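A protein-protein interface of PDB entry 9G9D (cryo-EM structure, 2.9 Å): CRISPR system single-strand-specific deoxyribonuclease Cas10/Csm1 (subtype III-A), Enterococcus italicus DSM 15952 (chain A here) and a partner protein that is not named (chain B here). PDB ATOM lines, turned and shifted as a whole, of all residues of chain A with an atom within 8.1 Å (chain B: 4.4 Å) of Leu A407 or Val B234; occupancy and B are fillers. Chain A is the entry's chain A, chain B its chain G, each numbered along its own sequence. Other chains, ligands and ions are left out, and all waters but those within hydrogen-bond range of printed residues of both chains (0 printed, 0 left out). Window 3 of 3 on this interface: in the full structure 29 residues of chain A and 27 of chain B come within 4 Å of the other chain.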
ATOM      1  N   LYS A 354      21.322  -6.222  24.775  1.00  0.00           N
ATOM      2  CA  LYS A 354      22.384  -5.302  25.167  1.00  0.00           C
ATOM      3  C   LYS A 354      21.841  -4.197  26.064  1.00  0.00           C
ATOM      4  O   LYS A 354      22.502  -3.785  27.024  1.00  0.00           O
ATOM      5  CB  LYS A 354      23.053  -4.710  23.928  1.00  0.00           C
ATOM      6  CG  LYS A 354      24.344  -3.961  24.207  1.00  0.00           C
ATOM      7  CD  LYS A 354      25.035  -3.578  22.909  1.00  0.00           C
ATOM      8  CE  LYS A 354      26.392  -2.951  23.167  1.00  0.00           C
ATOM      9  NZ  LYS A 354      27.043  -2.507  21.904  1.00  0.00           N
ATOM     10  N   HIS A 403      34.854  -3.634  21.912  1.00  0.00           N
ATOM     11  CA  HIS A 403      34.069  -2.405  21.940  1.00  0.00           C
ATOM     12  C   HIS A 403      32.984  -2.482  23.007  1.00  0.00           C
ATOM     13  O   HIS A 403      33.003  -1.724  23.985  1.00  0.00           O
ATOM     14  CB  HIS A 403      33.461  -2.153  20.562  1.00  0.00           C
ATOM     15  CG  HIS A 403      33.299  -0.705  20.226  1.00  0.00           C
ATOM     16  ND1 HIS A 403      32.126  -0.016  20.442  1.00  0.00           N
ATOM     17  CD2 HIS A 403      34.162   0.183  19.679  1.00  0.00           C
ATOM     18  CE1 HIS A 403      32.274   1.235  20.045  1.00  0.00           C
ATOM     19  NE2 HIS A 403      33.501   1.382  19.580  1.00  0.00           N
ATOM     20  N   TYR A 405      30.223  -1.553  23.838  1.00  0.00           N
ATOM     21  CA  TYR A 405      29.322  -0.481  24.243  1.00  0.00           C
ATOM     22  C   TYR A 405      29.361   0.619  23.193  1.00  0.00           C
ATOM     23  O   TYR A 405      30.318   0.739  22.426  1.00  0.00           O
ATOM     24  CB  TYR A 405      29.678   0.066  25.631  1.00  0.00           C
ATOM     25  CG  TYR A 405      29.322  -0.880  26.754  1.00  0.00           C
ATOM     26  CD1 TYR A 405      27.996  -1.125  27.083  1.00  0.00           C
ATOM     27  CD2 TYR A 405      30.307  -1.541  27.471  1.00  0.00           C
ATOM     28  CE1 TYR A 405      27.662  -1.997  28.098  1.00  0.00           C
ATOM     29  CE2 TYR A 405      29.984  -2.414  28.490  1.00  0.00           C
ATOM     30  CZ  TYR A 405      28.660  -2.639  28.799  1.00  0.00           C
ATOM     31  OH  TYR A 405      28.331  -3.507  29.813  1.00  0.00           O
ATOM     32  N   SER A 406      28.302   1.425  23.173  1.00  0.00           N
ATOM     33  CA  SER A 406      28.136   2.473  22.179  1.00  0.00           C
ATOM     34  C   SER A 406      28.241   3.841  22.839  1.00  0.00           C
ATOM     35  O   SER A 406      28.317   3.960  24.063  1.00  0.00           O
ATOM     36  CB  SER A 406      26.792   2.346  21.450  1.00  0.00           C
ATOM     37  OG  SER A 406      26.629   3.386  20.504  1.00  0.00           O
ATOM     38  N   LEU A 407      28.242   4.879  21.997  1.00  0.00           N
ATOM     39  CA  LEU A 407      28.385   6.243  22.496  1.00  0.00           C
ATOM     40  C   LEU A 407      27.240   6.622  23.428  1.00  0.00           C
ATOM     41  O   LEU A 407      27.468   7.177  24.509  1.00  0.00           O
ATOM     42  CB  LEU A 407      28.465   7.220  21.324  1.00  0.00           C
ATOM     43  CG  LEU A 407      28.301   8.703  21.660  1.00  0.00           C
ATOM     44  CD1 LEU A 407      29.401   9.169  22.596  1.00  0.00           C
ATOM     45  CD2 LEU A 407      28.286   9.535  20.390  1.00  0.00           C
ATOM     46  N   ASN A 408      26.000   6.333  23.027  1.00  0.00           N
ATOM     47  CA  ASN A 408      24.857   6.677  23.868  1.00  0.00           C
ATOM     48  C   ASN A 408      24.857   5.865  25.156  1.00  0.00           C
ATOM     49  O   ASN A 408      24.492   6.376  26.221  1.00  0.00           O
ATOM     50  CB  ASN A 408      23.555   6.472  23.095  1.00  0.00           C
ATOM     51  CG  ASN A 408      23.435   7.398  21.902  1.00  0.00           C
ATOM     52  OD1 ASN A 408      24.027   8.477  21.878  1.00  0.00           O
ATOM     53  ND2 ASN A 408      22.663   6.982  20.904  1.00  0.00           N
ATOM     54  N   GLU A 409      25.252   4.593  25.076  1.00  0.00           N
ATOM     55  CA  GLU A 409      25.335   3.765  26.275  1.00  0.00           C
ATOM     56  C   GLU A 409      26.386   4.296  27.242  1.00  0.00           C
ATOM     57  O   GLU A 409      26.182   4.279  28.462  1.00  0.00           O
ATOM     58  CB  GLU A 409      25.637   2.320  25.886  1.00  0.00           C
ATOM     59  CG  GLU A 409      24.567   1.689  25.015  1.00  0.00           C
ATOM     60  CD  GLU A 409      25.004   0.371  24.417  1.00  0.00           C
ATOM     61  OE1 GLU A 409      26.175   0.267  23.998  1.00  0.00           O
ATOM     62  OE2 GLU A 409      24.178  -0.566  24.370  1.00  0.00           O
ATOM     63  N   ILE A 410      27.521   4.764  26.718  1.00  0.00           N
ATOM     64  CA  ILE A 410      28.562   5.325  27.575  1.00  0.00           C
ATOM     65  C   ILE A 410      28.063   6.588  28.267  1.00  0.00           C
ATOM     66  O   ILE A 410      28.233   6.755  29.482  1.00  0.00           O
ATOM     67  CB  ILE A 410      29.841   5.596  26.761  1.00  0.00           C
ATOM     68  CG1 ILE A 410      30.538   4.283  26.401  1.00  0.00           C
ATOM     69  CG2 ILE A 410      30.782   6.501  27.536  1.00  0.00           C
ATOM     70  CD1 ILE A 410      31.808   4.470  25.601  1.00  0.00           C
ATOM     71  N   LYS A 411      27.442   7.496  27.511  1.00  0.00           N
ATOM     72  CA  LYS A 411      26.943   8.733  28.105  1.00  0.00           C
ATOM     73  C   LYS A 411      25.849   8.452  29.127  1.00  0.00           C
ATOM     74  O   LYS A 411      25.643   9.237  30.059  1.00  0.00           O
ATOM     75  CB  LYS A 411      26.427   9.674  27.016  1.00  0.00           C
ATOM     76  CG  LYS A 411      27.483  10.114  26.017  1.00  0.00           C
ATOM     77  CD  LYS A 411      27.013  11.317  25.211  1.00  0.00           C
ATOM     78  CE  LYS A 411      25.680  11.049  24.529  1.00  0.00           C
ATOM     79  NZ  LYS A 411      25.772   9.938  23.545  1.00  0.00           N
ATOM     80  N   LEU A 412      25.131   7.339  28.964  1.00  0.00           N
ATOM     81  CA  LEU A 412      24.122   6.958  29.945  1.00  0.00           C
ATOM     82  C   LEU A 412      24.754   6.645  31.295  1.00  0.00           C
ATOM     83  O   LEU A 412      24.217   7.017  32.344  1.00  0.00           O
ATOM     84  CB  LEU A 412      23.324   5.759  29.433  1.00  0.00           C
ATOM     85  CG  LEU A 412      22.428   5.032  30.439  1.00  0.00           C
ATOM     86  CD1 LEU A 412      21.314   5.942  30.940  1.00  0.00           C
ATOM     87  CD2 LEU A 412      21.859   3.757  29.827  1.00  0.00           C
ATOM     88  N   PHE A 413      25.901   5.963  31.286  1.00  0.00           N
ATOM     89  CA  PHE A 413      26.532   5.534  32.531  1.00  0.00           C
ATOM     90  C   PHE A 413      26.947   6.722  33.390  1.00  0.00           C
ATOM     91  O   PHE A 413      26.801   6.690  34.617  1.00  0.00           O
ATOM     92  CB  PHE A 413      27.738   4.650  32.220  1.00  0.00           C
ATOM     93  CG  PHE A 413      27.375   3.301  31.676  1.00  0.00           C
ATOM     94  CD1 PHE A 413      26.350   2.564  32.245  1.00  0.00           C
ATOM     95  CD2 PHE A 413      28.054   2.771  30.592  1.00  0.00           C
ATOM     96  CE1 PHE A 413      26.015   1.322  31.748  1.00  0.00           C
ATOM     97  CE2 PHE A 413      27.721   1.530  30.091  1.00  0.00           C
ATOM     98  CZ  PHE A 413      26.700   0.805  30.669  1.00  0.00           C
ATOM     99  N   ASN A 414      27.473   7.777  32.767  1.00  0.00           N
ATOM    100  CA  ASN A 414      27.976   8.907  33.541  1.00  0.00           C
ATOM    101  C   ASN A 414      26.908   9.977  33.726  1.00  0.00           C
ATOM    102  O   ASN A 414      27.182  11.050  34.277  1.00  0.00           O
ATOM    103  CB  ASN A 414      29.215   9.488  32.863  1.00  0.00           C
ATOM    104  CG  ASN A 414      30.262   8.434  32.566  1.00  0.00           C
ATOM    105  OD1 ASN A 414      31.023   8.035  33.446  1.00  0.00           O
ATOM    106  ND2 ASN A 414      30.305   7.976  31.320  1.00  0.00           N
ATOM    107  N   ASP B 230      31.570  14.433  25.991  1.00  0.00           N
ATOM    108  CA  ASP B 230      30.673  13.919  24.960  1.00  0.00           C
ATOM    109  C   ASP B 230      31.095  14.389  23.574  1.00  0.00           C
ATOM    110  O   ASP B 230      31.084  13.608  22.612  1.00  0.00           O
ATOM    111  CB  ASP B 230      29.240  14.350  25.260  1.00  0.00           C
ATOM    112  CG  ASP B 230      28.890  14.213  26.727  1.00  0.00           C
ATOM    113  OD1 ASP B 230      29.434  13.302  27.386  1.00  0.00           O
ATOM    114  OD2 ASP B 230      28.075  15.019  27.223  1.00  0.00           O
ATOM    115  N   GLU B 231      31.478  15.662  23.453  1.00  0.00           N
ATOM    116  CA  GLU B 231      31.910  16.189  22.163  1.00  0.00           C
ATOM    117  C   GLU B 231      33.140  15.449  21.653  1.00  0.00           C
ATOM    118  O   GLU B 231      33.216  15.099  20.470  1.00  0.00           O
ATOM    119  CB  GLU B 231      32.192  17.688  22.274  1.00  0.00           C
ATOM    120  CG  GLU B 231      31.031  18.514  22.815  1.00  0.00           C
ATOM    121  CD  GLU B 231      30.937  18.476  24.329  1.00  0.00           C
ATOM    122  OE1 GLU B 231      31.917  18.051  24.975  1.00  0.00           O
ATOM    123  OE2 GLU B 231      29.884  18.868  24.873  1.00  0.00           O
ATOM    124  N   GLU B 232      34.112  15.197  22.532  1.00  0.00           N
ATOM    125  CA  GLU B 232      35.268  14.402  22.136  1.00  0.00           C
ATOM    126  C   GLU B 232      34.898  12.931  21.994  1.00  0.00           C
ATOM    127  O   GLU B 232      35.515  12.201  21.208  1.00  0.00           O
ATOM    128  CB  GLU B 232      36.398  14.578  23.151  1.00  0.00           C
ATOM    129  CG  GLU B 232      36.700  16.024  23.504  1.00  0.00           C
ATOM    130  CD  GLU B 232      37.926  16.160  24.382  1.00  0.00           C
ATOM    131  OE1 GLU B 232      38.895  15.402  24.171  1.00  0.00           O
ATOM    132  OE2 GLU B 232      37.918  17.019  25.289  1.00  0.00           O
ATOM    133  N   LEU B 233      33.900  12.477  22.759  1.00  0.00           N
ATOM    134  CA  LEU B 233      33.469  11.084  22.684  1.00  0.00           C
ATOM    135  C   LEU B 233      32.941  10.743  21.300  1.00  0.00           C
ATOM    136  O   LEU B 233      33.224   9.660  20.771  1.00  0.00           O
ATOM    137  CB  LEU B 233      32.401  10.804  23.740  1.00  0.00           C
ATOM    138  CG  LEU B 233      32.861  10.183  25.058  1.00  0.00           C
ATOM    139  CD1 LEU B 233      31.723  10.180  26.065  1.00  0.00           C
ATOM    140  CD2 LEU B 233      33.373   8.773  24.823  1.00  0.00           C
ATOM    141  N   VAL B 234      32.180  11.661  20.695  1.00  0.00           N
ATOM    142  CA  VAL B 234      31.590  11.404  19.382  1.00  0.00           C
ATOM    143  C   VAL B 234      32.666  11.020  18.375  1.00  0.00           C
ATOM    144  O   VAL B 234      32.503  10.068  17.601  1.00  0.00           O
ATOM    145  CB  VAL B 234      30.786  12.629  18.908  1.00  0.00           C
ATOM    146  CG1 VAL B 234      30.272  12.414  17.494  1.00  0.00           C
ATOM    147  CG2 VAL B 234      29.633  12.914  19.854  1.00  0.00           C
ATOM    148  N   ASP B 235      33.786  11.745  18.373  1.00  0.00           N
ATOM    149  CA  ASP B 235      34.832  11.478  17.393  1.00  0.00           C
ATOM    150  C   ASP B 235      35.732  10.324  17.823  1.00  0.00           C
ATOM    151  O   ASP B 235      36.154   9.516  16.988  1.00  0.00           O
ATOM    152  CB  ASP B 235      35.658  12.740  17.156  1.00  0.00           C
ATOM    153  CG  ASP B 235      34.814  13.903  16.676  1.00  0.00           C
ATOM    154  OD1 ASP B 235      34.082  14.489  17.501  1.00  0.00           O
ATOM    155  OD2 ASP B 235      34.877  14.227  15.472  1.00  0.00           O
ATOM    156  N   CYS B 236      36.036  10.224  19.120  1.00  0.00           N
ATOM    157  CA  CYS B 236      37.038   9.258  19.563  1.00  0.00           C
ATOM    158  C   CYS B 236      36.484   7.839  19.593  1.00  0.00           C
ATOM    159  O   CYS B 236      37.220   6.875  19.353  1.00  0.00           O
ATOM    160  CB  CYS B 236      37.570   9.648  20.941  1.00  0.00           C
ATOM    161  SG  CYS B 236      36.482   9.203  22.313  1.00  0.00           S
ATOM    162  N   LEU B 237      35.231   7.677  20.017  1.00  0.00           N
ATOM    163  CA  LEU B 237      34.715   6.297  20.241  1.00  0.00           C
ATOM    164  C   LEU B 237      34.856   5.393  19.009  1.00  0.00           C
ATOM    165  O   LEU B 237      35.168   4.197  19.195  1.00  0.00           O
ATOM    166  CB  LEU B 237      33.276   6.354  20.744  1.00  0.00           C
ATOM    167  CG  LEU B 237      33.160   6.243  22.264  1.00  0.00           C
ATOM    168  CD1 LEU B 237      31.715   6.241  22.675  1.00  0.00           C
ATOM    169  CD2 LEU B 237      33.857   4.972  22.713  1.00  0.00           C
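The backbone carbonyl oxygen of Leu A407 sits close to the side-chain amino group of Lys A411, at 3.4 Å. NZ of Lys A411 is in hydrogen-bond range of OD1 of Asn A408 (2.8 Å). The backbone carbonyl oxygen of Tyr A405 lies within hydrogen-bond range of a ring nitrogen (ND1) of His A403. The backbone carbonyl oxygen of Leu B233 lies close to the side-chain sulfur of Cys B236, 3.6 Å away. The backbone carbonyl oxygen (O) of Ile A410 lies within hydrogen-bond range of the side-chain amide nitrogen (ND2) of Asn A414 (3.0 Å).
NE2 of His A403 is in hydrogen-bond range of O of Leu B237 (3.3 Å).
Among the printed residues, pairs that only touch across the chains: Leu A407 with Leu B233, Leu A407 with Val B234, Leu A407 with Leu B237, Ile A410 with Leu B237 and Lys A411 with Asp B230.
Of the printed residues of chain B, His A403 touches Leu B237 (3.3 Å). Of chain B, only Leu B233 (3.6 Å), Val B234 (3.7 Å) and Leu B237 (3.3 Å) come within 4 Å of Leu A407. Of the printed residues of chain B, Lys A411 touches Asp B230. Printed residues of chain A within 4 Å of Asp B230: Lys A411. Of the printed residues of chain A, Leu B233 touches Leu A407. Of chain A, only Leu A407 (3.7 Å) comes within 4 Å of Val B234. Of the printed residues of chain A, Leu B237 touches His A403, Leu A407 and Ile A410. The nearest residue of chain A that does not touch Val B234 is Lys A411 (6.1 Å). The nearest printed residue of chain A that does not touch Asp B230 is Leu A407 (4.7 Å).
Of the 12 printed residues of chain A, 4 touch a printed residue of chain B. Hydrophobic or aromatic side chains of chain A within 4 Å of the printed part of chain B: His A403, Leu A407 and Ile A410. Hydrophobic or aromatic side chains of chain B within 4 Å of the printed part of chain A: Leu B233, Val B234 and Leu B237. Among the printed residues, 6 pairs touch across the chains. Among the printed residues, no Asp or Glu carboxylate lies within 4 Å of a Lys or Arg side-chain nitrogen of the other chain.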
